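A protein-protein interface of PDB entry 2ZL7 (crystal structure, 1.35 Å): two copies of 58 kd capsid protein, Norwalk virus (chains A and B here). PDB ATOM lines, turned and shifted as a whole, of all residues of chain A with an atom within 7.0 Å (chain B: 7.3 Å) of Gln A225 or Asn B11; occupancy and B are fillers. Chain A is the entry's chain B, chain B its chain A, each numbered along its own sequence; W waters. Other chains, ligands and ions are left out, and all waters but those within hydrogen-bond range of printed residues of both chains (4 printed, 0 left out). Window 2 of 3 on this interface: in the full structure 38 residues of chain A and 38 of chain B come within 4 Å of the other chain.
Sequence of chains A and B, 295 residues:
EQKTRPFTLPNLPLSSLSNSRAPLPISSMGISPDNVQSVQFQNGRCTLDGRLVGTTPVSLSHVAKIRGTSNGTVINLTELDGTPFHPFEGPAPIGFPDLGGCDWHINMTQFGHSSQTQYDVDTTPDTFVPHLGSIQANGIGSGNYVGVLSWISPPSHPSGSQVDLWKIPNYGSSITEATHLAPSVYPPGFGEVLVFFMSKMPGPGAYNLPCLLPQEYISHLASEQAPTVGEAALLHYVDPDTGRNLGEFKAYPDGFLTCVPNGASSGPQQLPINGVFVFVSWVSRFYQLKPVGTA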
ATOM      1  N   LEU A  48      -9.193  10.897 -26.483  1.00  0.00           N
ATOM      2  CA  LEU A  48      -9.168  12.143 -25.727  1.00  0.00           C
ATOM      3  C   LEU A  48      -9.266  11.966 -24.214  1.00  0.00           C
ATOM      4  O   LEU A  48      -8.810  12.822 -23.470  1.00  0.00           O
ATOM      5  CB  LEU A  48     -10.229  13.131 -26.216  1.00  0.00           C
ATOM      6  CG  LEU A  48     -10.095  13.568 -27.673  1.00  0.00           C
ATOM      7  CD1 LEU A  48     -11.175  14.616 -27.994  1.00  0.00           C
ATOM      8  CD2 LEU A  48      -8.703  14.117 -27.999  1.00  0.00           C
ATOM      9  N   ASP A  49      -9.857  10.857 -23.765  1.00  0.00           N
ATOM     10  CA  ASP A  49      -9.925  10.556 -22.343  1.00  0.00           C
ATOM     11  C   ASP A  49      -8.729   9.763 -21.806  1.00  0.00           C
ATOM     12  O   ASP A  49      -8.695   9.399 -20.642  1.00  0.00           O
ATOM     13  CB  ASP A  49     -11.277   9.910 -21.968  1.00  0.00           C
ATOM     14  CG  ASP A  49     -11.447   8.480 -22.451  1.00  0.00           C
ATOM     15  OD1 ASP A  49     -10.502   7.870 -23.001  1.00  0.00           O
ATOM     16  OD2 ASP A  49     -12.563   7.930 -22.230  1.00  0.00           O
ATOM     17  N   GLY A  50      -7.716   9.561 -22.653  1.00  0.00           N
ATOM     18  CA  GLY A  50      -6.479   8.965 -22.208  1.00  0.00           C
ATOM     19  C   GLY A  50      -6.302   7.483 -22.397  1.00  0.00           C
ATOM     20  O   GLY A  50      -5.423   6.906 -21.770  1.00  0.00           O
ATOM     21  N   ARG A  51      -7.101   6.862 -23.262  1.00  0.00           N
ATOM     22  CA  ARG A  51      -6.958   5.428 -23.554  1.00  0.00           C
ATOM     23  C   ARG A  51      -5.919   5.215 -24.656  1.00  0.00           C
ATOM     24  O   ARG A  51      -6.134   5.606 -25.795  1.00  0.00           O
ATOM     25  CB  ARG A  51      -8.306   4.873 -24.008  1.00  0.00           C
ATOM     26  CG  ARG A  51      -8.371   3.363 -24.204  1.00  0.00           C
ATOM     27  CD  ARG A  51      -9.734   3.023 -24.766  1.00  0.00           C
ATOM     28  NE  ARG A  51      -9.913   1.620 -25.119  1.00  0.00           N
ATOM     29  CZ  ARG A  51     -10.363   0.681 -24.290  1.00  0.00           C
ATOM     30  NH1 ARG A  51     -10.651   0.952 -23.016  1.00  0.00           N
ATOM     31  NH2 ARG A  51     -10.487  -0.558 -24.749  1.00  0.00           N
ATOM     32  N   SER A 219       1.144  11.551 -23.948  1.00  0.00           N
ATOM     33  CA  SER A 219       1.444  11.480 -22.542  1.00  0.00           C
ATOM     34  C   SER A 219       0.560  12.452 -21.768  1.00  0.00           C
ATOM     35  O   SER A 219       0.128  12.129 -20.661  1.00  0.00           O
ATOM     36  CB  SER A 219       2.931  11.702 -22.251  1.00  0.00           C
ATOM     37  OG  SER A 219       3.409  12.897 -22.842  1.00  0.00           O
ATOM     38  N   HIS A 220       0.260  13.620 -22.346  1.00  0.00           N
ATOM     39  CA  HIS A 220      -0.632  14.583 -21.684  1.00  0.00           C
ATOM     40  C   HIS A 220      -2.019  14.008 -21.483  1.00  0.00           C
ATOM     41  O   HIS A 220      -2.568  14.106 -20.402  1.00  0.00           O
ATOM     42  CB  HIS A 220      -0.734  15.843 -22.535  1.00  0.00           C
ATOM     43  CG  HIS A 220      -1.455  16.978 -21.883  1.00  0.00           C
ATOM     44  ND1 HIS A 220      -2.810  17.198 -21.997  1.00  0.00           N
ATOM     45  CD2 HIS A 220      -0.963  18.004 -21.155  1.00  0.00           C
ATOM     46  CE1 HIS A 220      -3.123  18.283 -21.309  1.00  0.00           C
ATOM     47  NE2 HIS A 220      -2.018  18.807 -20.818  1.00  0.00           N
ATOM     48  N   LEU A 221      -2.605  13.454 -22.534  1.00  0.00           N
ATOM     49  CA  LEU A 221      -3.962  12.900 -22.432  1.00  0.00           C
ATOM     50  C   LEU A 221      -4.009  11.711 -21.502  1.00  0.00           C
ATOM     51  O   LEU A 221      -4.974  11.539 -20.758  1.00  0.00           O
ATOM     52  CB  LEU A 221      -4.491  12.506 -23.814  1.00  0.00           C
ATOM     53  CG  LEU A 221      -4.704  13.654 -24.806  1.00  0.00           C
ATOM     54  CD1 LEU A 221      -4.910  13.115 -26.217  1.00  0.00           C
ATOM     55  CD2 LEU A 221      -5.844  14.570 -24.378  1.00  0.00           C
ATOM     56  N   ALA A 222      -2.974  10.879 -21.537  1.00  0.00           N
ATOM     57  CA  ALA A 222      -2.923   9.711 -20.661  1.00  0.00           C
ATOM     58  C   ALA A 222      -2.798  10.105 -19.189  1.00  0.00           C
ATOM     59  O   ALA A 222      -3.282   9.396 -18.311  1.00  0.00           O
ATOM     60  CB  ALA A 222      -1.783   8.781 -21.083  1.00  0.00           C
ATOM     61  N   SER A 223      -2.117  11.212 -18.923  1.00  0.00           N
ATOM     62  CA  SER A 223      -2.005  11.738 -17.554  1.00  0.00           C
ATOM     63  C   SER A 223      -3.325  12.394 -17.129  1.00  0.00           C
ATOM     64  O   SER A 223      -3.807  12.178 -16.023  1.00  0.00           O
ATOM     65  CB  SER A 223      -0.861  12.743 -17.474  1.00  0.00           C
ATOM     66  OG  SER A 223      -0.916  13.492 -16.268  1.00  0.00           O
ATOM     67  N   GLU A 224      -3.913  13.182 -18.028  1.00  0.00           N
ATOM     68  CA  GLU A 224      -5.101  13.989 -17.726  1.00  0.00           C
ATOM     69  C   GLU A 224      -6.324  13.135 -17.435  1.00  0.00           C
ATOM     70  O   GLU A 224      -7.120  13.463 -16.538  1.00  0.00           O
ATOM     71  CB  GLU A 224      -5.382  14.898 -18.921  1.00  0.00           C
ATOM     72  CG  GLU A 224      -6.629  15.760 -18.818  1.00  0.00           C
ATOM     73  CD  GLU A 224      -6.797  16.725 -19.980  1.00  0.00           C
ATOM     74  OE1 GLU A 224      -5.970  16.726 -20.926  1.00  0.00           O
ATOM     75  OE2 GLU A 224      -7.771  17.490 -19.971  1.00  0.00           O
ATOM     76  N   GLN A 225      -6.518  12.055 -18.195  1.00  0.00           N
ATOM     77  CA  GLN A 225      -7.626  11.135 -17.975  1.00  0.00           C
ATOM     78  C   GLN A 225      -8.950  11.899 -17.887  1.00  0.00           C
ATOM     79  O   GLN A 225      -9.738  11.699 -16.956  1.00  0.00           O
ATOM     80  CB  GLN A 225      -7.359  10.282 -16.738  1.00  0.00           C
ATOM     81  CG  GLN A 225      -6.151   9.389 -16.957  1.00  0.00           C
ATOM     82  CD  GLN A 225      -5.660   8.719 -15.717  1.00  0.00           C
ATOM     83  OE1 GLN A 225      -6.426   8.480 -14.785  1.00  0.00           O
ATOM     84  NE2 GLN A 225      -4.356   8.418 -15.682  1.00  0.00           N
ATOM     85  N   ALA A 226      -9.181  12.779 -18.855  1.00  0.00           N
ATOM     86  CA  ALA A 226     -10.340  13.684 -18.866  1.00  0.00           C
ATOM     87  C   ALA A 226     -11.645  12.945 -18.536  1.00  0.00           C
ATOM     88  O   ALA A 226     -11.978  11.960 -19.188  1.00  0.00           O
ATOM     89  CB  ALA A 226     -10.454  14.369 -20.217  1.00  0.00           C
ATOM     90  N   PRO A 227     -12.361  13.395 -17.483  1.00  0.00           N
ATOM     91  CA  PRO A 227     -13.591  12.749 -17.044  1.00  0.00           C
ATOM     92  C   PRO A 227     -14.846  13.137 -17.831  1.00  0.00           C
ATOM     93  O   PRO A 227     -15.854  12.441 -17.697  1.00  0.00           O
ATOM     94  CB  PRO A 227     -13.711  13.210 -15.592  1.00  0.00           C
ATOM     95  CG  PRO A 227     -13.098  14.560 -15.587  1.00  0.00           C
ATOM     96  CD  PRO A 227     -11.998  14.529 -16.616  1.00  0.00           C
ATOM     97  N   THR A 228     -14.787  14.210 -18.630  1.00  0.00           N
ATOM     98  CA  THR A 228     -15.979  14.828 -19.259  1.00  0.00           C
ATOM     99  C   THR A 228     -15.815  15.137 -20.760  1.00  0.00           C
ATOM    100  O   THR A 228     -16.065  16.261 -21.207  1.00  0.00           O
ATOM    101  CB  THR A 228     -16.355  16.180 -18.550  1.00  0.00           C
ATOM    102  OG1 THR A 228     -15.938  16.164 -17.181  1.00  0.00           O
ATOM    103  CG2 THR A 228     -17.853  16.427 -18.616  1.00  0.00           C
ATOM    104  N   VAL A 229     -15.408  14.139 -21.545  1.00  0.00           N
ATOM    105  CA  VAL A 229     -15.202  14.335 -22.981  1.00  0.00           C
ATOM    106  C   VAL A 229     -16.553  14.406 -23.696  1.00  0.00           C
ATOM    107  O   VAL A 229     -17.419  13.569 -23.453  1.00  0.00           O
ATOM    108  CB  VAL A 229     -14.335  13.204 -23.583  1.00  0.00           C
ATOM    109  CG1 VAL A 229     -14.241  13.324 -25.118  1.00  0.00           C
ATOM    110  CG2 VAL A 229     -12.930  13.227 -22.953  1.00  0.00           C
ATOM    111  N   THR B   8       0.248  20.512 -10.565  1.00  0.00           N
ATOM    112  CA  THR B   8       0.278  19.076 -10.844  1.00  0.00           C
ATOM    113  C   THR B   8       1.611  18.585 -11.410  1.00  0.00           C
ATOM    114  O   THR B   8       2.353  19.321 -12.085  1.00  0.00           O
ATOM    115  CB  THR B   8      -0.810  18.655 -11.848  1.00  0.00           C
ATOM    116  OG1 THR B   8      -0.546  19.248 -13.115  1.00  0.00           O
ATOM    117  CG2 THR B   8      -2.204  19.087 -11.379  1.00  0.00           C
ATOM    118  N   LEU B   9       1.891  17.317 -11.106  1.00  0.00           N
ATOM    119  CA  LEU B   9       2.893  16.529 -11.820  1.00  0.00           C
ATOM    120  C   LEU B   9       2.136  15.489 -12.643  1.00  0.00           C
ATOM    121  O   LEU B   9       0.958  15.231 -12.381  1.00  0.00           O
ATOM    122  CB  LEU B   9       3.823  15.834 -10.830  1.00  0.00           C
ATOM    123  CG  LEU B   9       4.680  16.803 -10.004  1.00  0.00           C
ATOM    124  CD1 LEU B   9       5.396  16.043  -8.905  1.00  0.00           C
ATOM    125  CD2 LEU B   9       5.668  17.584 -10.872  1.00  0.00           C
ATOM    126  N   PRO B  10       2.781  14.905 -13.663  1.00  0.00           N
ATOM    127  CA  PRO B  10       2.101  13.892 -14.465  1.00  0.00           C
ATOM    128  C   PRO B  10       1.527  12.730 -13.656  1.00  0.00           C
ATOM    129  O   PRO B  10       2.183  12.181 -12.768  1.00  0.00           O
ATOM    130  CB  PRO B  10       3.207  13.369 -15.389  1.00  0.00           C
ATOM    131  CG  PRO B  10       4.158  14.509 -15.516  1.00  0.00           C
ATOM    132  CD  PRO B  10       4.145  15.189 -14.162  1.00  0.00           C
ATOM    133  N   ASN B  11       0.291  12.375 -13.974  1.00  0.00           N
ATOM    134  CA  ASN B  11      -0.361  11.232 -13.353  1.00  0.00           C
ATOM    135  C   ASN B  11      -0.014   9.992 -14.172  1.00  0.00           C
ATOM    136  O   ASN B  11      -0.866   9.407 -14.850  1.00  0.00           O
ATOM    137  CB  ASN B  11      -1.875  11.444 -13.276  1.00  0.00           C
ATOM    138  CG  ASN B  11      -2.578  10.340 -12.543  1.00  0.00           C
ATOM    139  OD1 ASN B  11      -1.985   9.582 -11.806  1.00  0.00           O
ATOM    140  ND2 ASN B  11      -3.882  10.232 -12.774  1.00  0.00           N
ATOM    141  N   LEU B  12       1.258   9.630 -14.114  1.00  0.00           N
ATOM    142  CA  LEU B  12       1.813   8.535 -14.902  1.00  0.00           C
ATOM    143  C   LEU B  12       2.842   7.809 -14.057  1.00  0.00           C
ATOM    144  O   LEU B  12       3.627   8.462 -13.355  1.00  0.00           O
ATOM    145  CB  LEU B  12       2.505   9.074 -16.152  1.00  0.00           C
ATOM    146  CG  LEU B  12       1.607   9.805 -17.156  1.00  0.00           C
ATOM    147  CD1 LEU B  12       2.452  10.514 -18.186  1.00  0.00           C
ATOM    148  CD2 LEU B  12       0.615   8.846 -17.815  1.00  0.00           C
ATOM    149  N   PRO B  13       2.863   6.470 -14.110  1.00  0.00           N
ATOM    150  CA  PRO B  13       3.850   5.764 -13.313  1.00  0.00           C
ATOM    151  C   PRO B  13       5.269   5.992 -13.830  1.00  0.00           C
ATOM    152  O   PRO B  13       5.486   6.067 -15.047  1.00  0.00           O
ATOM    153  CB  PRO B  13       3.425   4.302 -13.442  1.00  0.00           C
ATOM    154  CG  PRO B  13       2.599   4.221 -14.637  1.00  0.00           C
ATOM    155  CD  PRO B  13       1.999   5.561 -14.881  1.00  0.00           C
ATOM    156  N   LEU B  17       7.933   6.203 -18.068  1.00  0.00           N
ATOM    157  CA  LEU B  17       8.521   7.471 -18.505  1.00  0.00           C
ATOM    158  C   LEU B  17       9.953   7.322 -18.968  1.00  0.00           C
ATOM    159  O   LEU B  17      10.541   6.240 -18.903  1.00  0.00           O
ATOM    160  CB  LEU B  17       8.416   8.478 -17.361  1.00  0.00           C
ATOM    161  CG  LEU B  17       7.001   8.709 -16.815  1.00  0.00           C
ATOM    162  CD1 LEU B  17       6.998   9.790 -15.721  1.00  0.00           C
ATOM    163  CD2 LEU B  17       6.006   9.064 -17.898  1.00  0.00           C
ATOM    164  N   TYR B 217       7.983  14.802 -17.316  1.00  0.00           N
ATOM    165  CA  TYR B 217       7.768  15.852 -16.306  1.00  0.00           C
ATOM    166  C   TYR B 217       8.135  17.218 -16.890  1.00  0.00           C
ATOM    167  O   TYR B 217       7.499  18.221 -16.593  1.00  0.00           O
ATOM    168  CB  TYR B 217       8.616  15.590 -15.063  1.00  0.00           C
ATOM    169  CG  TYR B 217       8.028  14.619 -14.053  1.00  0.00           C
ATOM    170  CD1 TYR B 217       7.369  13.452 -14.432  1.00  0.00           C
ATOM    171  CD2 TYR B 217       8.180  14.856 -12.703  1.00  0.00           C
ATOM    172  CE1 TYR B 217       6.856  12.572 -13.480  1.00  0.00           C
ATOM    173  CE2 TYR B 217       7.674  13.979 -11.751  1.00  0.00           C
ATOM    174  CZ  TYR B 217       7.006  12.859 -12.147  1.00  0.00           C
ATOM    175  OH  TYR B 217       6.486  11.997 -11.197  1.00  0.00           O
ATOM    176  N   HIS B 220       5.483  18.405 -19.213  1.00  0.00           N
ATOM    177  CA  HIS B 220       4.317  18.752 -18.385  1.00  0.00           C
ATOM    178  C   HIS B 220       4.496  20.100 -17.717  1.00  0.00           C
ATOM    179  O   HIS B 220       3.623  20.960 -17.790  1.00  0.00           O
ATOM    180  CB  HIS B 220       4.117  17.666 -17.338  1.00  0.00           C
ATOM    181  CG  HIS B 220       2.866  17.804 -16.538  1.00  0.00           C
ATOM    182  ND1 HIS B 220       2.764  18.571 -15.399  1.00  0.00           N
ATOM    183  CD2 HIS B 220       1.657  17.234 -16.721  1.00  0.00           C
ATOM    184  CE1 HIS B 220       1.529  18.482 -14.928  1.00  0.00           C
ATOM    185  NE2 HIS B 220       0.842  17.676 -15.706  1.00  0.00           N
ATOM    186  N   PRO B 240      -0.722   3.511  -7.475  1.00  0.00           N
ATOM    187  CA  PRO B 240      -1.987   3.904  -8.121  1.00  0.00           C
ATOM    188  C   PRO B 240      -3.246   3.089  -7.770  1.00  0.00           C
ATOM    189  O   PRO B 240      -4.325   3.664  -7.582  1.00  0.00           O
ATOM    190  CB  PRO B 240      -1.687   3.769  -9.622  1.00  0.00           C
ATOM    191  CG  PRO B 240      -0.251   3.572  -9.761  1.00  0.00           C
ATOM    192  CD  PRO B 240       0.364   3.267  -8.442  1.00  0.00           C
ATOM    193  N   VAL B 276       3.447   6.808  -8.697  1.00  0.00           N
ATOM    194  CA  VAL B 276       3.132   8.105  -9.269  1.00  0.00           C
ATOM    195  C   VAL B 276       3.414   9.161  -8.212  1.00  0.00           C
ATOM    196  O   VAL B 276       2.996   9.017  -7.050  1.00  0.00           O
ATOM    197  CB  VAL B 276       1.641   8.170  -9.667  1.00  0.00           C
ATOM    198  CG1 VAL B 276       1.267   9.568 -10.085  1.00  0.00           C
ATOM    199  CG2 VAL B 276       1.333   7.168 -10.769  1.00  0.00           C
ATOM    200  N   PHE B 277       4.118  10.227  -8.572  1.00  0.00           N
ATOM    201  CA  PHE B 277       4.264  11.361  -7.655  1.00  0.00           C
ATOM    202  C   PHE B 277       3.043  12.245  -7.738  1.00  0.00           C
ATOM    203  O   PHE B 277       2.608  12.624  -8.828  1.00  0.00           O
ATOM    204  CB  PHE B 277       5.522  12.176  -7.957  1.00  0.00           C
ATOM    205  CG  PHE B 277       6.769  11.573  -7.423  1.00  0.00           C
ATOM    206  CD1 PHE B 277       6.988  11.512  -6.050  1.00  0.00           C
ATOM    207  CD2 PHE B 277       7.739  11.047  -8.273  1.00  0.00           C
ATOM    208  CE1 PHE B 277       8.138  10.984  -5.561  1.00  0.00           C
ATOM    209  CE2 PHE B 277       8.893  10.497  -7.764  1.00  0.00           C
ATOM    210  CZ  PHE B 277       9.090  10.471  -6.411  1.00  0.00           C
ATOM    211  N   VAL B 278       2.482  12.586  -6.576  1.00  0.00           N
ATOM    212  CA  VAL B 278       1.268  13.378  -6.488  1.00  0.00           C
ATOM    213  C   VAL B 278       1.548  14.603  -5.625  1.00  0.00           C
ATOM    214  O   VAL B 278       2.058  14.476  -4.503  1.00  0.00           O
ATOM    215  CB  VAL B 278       0.118  12.568  -5.852  1.00  0.00           C
ATOM    216  CG1 VAL B 278      -1.166  13.383  -5.788  1.00  0.00           C
ATOM    217  CG2 VAL B 278      -0.142  11.285  -6.631  1.00  0.00           C
HETATM  218  O   HOH W   1      -1.636  15.519 -13.598  1.00  0.00           O
HETATM  219  O   HOH W   2      -5.266  12.585 -13.810  1.00  0.00           O
HETATM  220  O   HOH W   3      -5.579   7.944 -12.367  1.00  0.00           O
HETATM  221  O   HOH W   4      -1.612   6.762 -15.104  1.00  0.00           O
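Of chain B, only Asn B11 (3.5 Å) comes within 4 Å of Gln A225.
Of chain A, only Ser A223 and Gln A225 come within 4 Å of Asn B11.
Of the printed residues of chain B, Ala A222 touches Leu B12.
Of the printed residues of chain B, Ser A219 touches Leu B12.
Printed residues of chain B within 4 Å of Ser A223: Pro B10 (3.5 Å), Asn B11 (2.8 Å) and Leu B12 (3.8 Å).
The nearest printed residue of chain B that does not touch Ser A223 is His B220 (4.6 Å).
NE2 of Gln A225 sits at hydrogen-bond distance from O of Ala A222.
Ser A219 touches Leu B12.
Ala A222 touches Leu B12 (C to CD2, 3.9 Å).
Pro B10 touches Ser A223 (CA to OG, 3.5 Å).
Leu B12 touches Ser A223 (CD2 to N, 3.8 Å).
Of the 13 printed residues of chain B, 3 touch a printed residue of chain A.
Printed residues of chain B that touch a printed residue of chain A: Pro B10, Asn B11 and Leu B12.
Hydrophobic or aromatic side chains of chain B that line the printed part of chain A: Leu B12.
Among the printed residues, 6 pairs touch across the chains.
Among the printed residues, no Asp or Glu carboxylate lies within 4 Å of a Lys or Arg side-chain nitrogen of the other chain.
Water W3 lies within hydrogen-bond range of the side-chain amide oxygen of Gln A225 and the side-chain amide nitrogen of Asn B11.
Water W2 lies within hydrogen-bond range of O of Ser A223 (2.7 Å), ND2 of Asn B11 (2.9 Å) and O of Glu A224 (3.4 Å).
Water W4 bridges O of Asn B11 and NE2 of Gln A225.
Water W1 lies within hydrogen-bond range of the backbone carbonyl oxygen of Leu B9 (2.9 Å) and the side-chain hydroxyl of Ser A223 (3.4 Å).
Position printed for both chains: 220.
The side-chain amide nitrogen of Asn B11 sits close to the side-chain amide nitrogen of Gln A225, 3.5 Å away.
The side-chain hydroxyl (OG) of Ser A223 lies within hydrogen-bond range of the backbone NH (N) of Asn B11 (2.8 Å).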
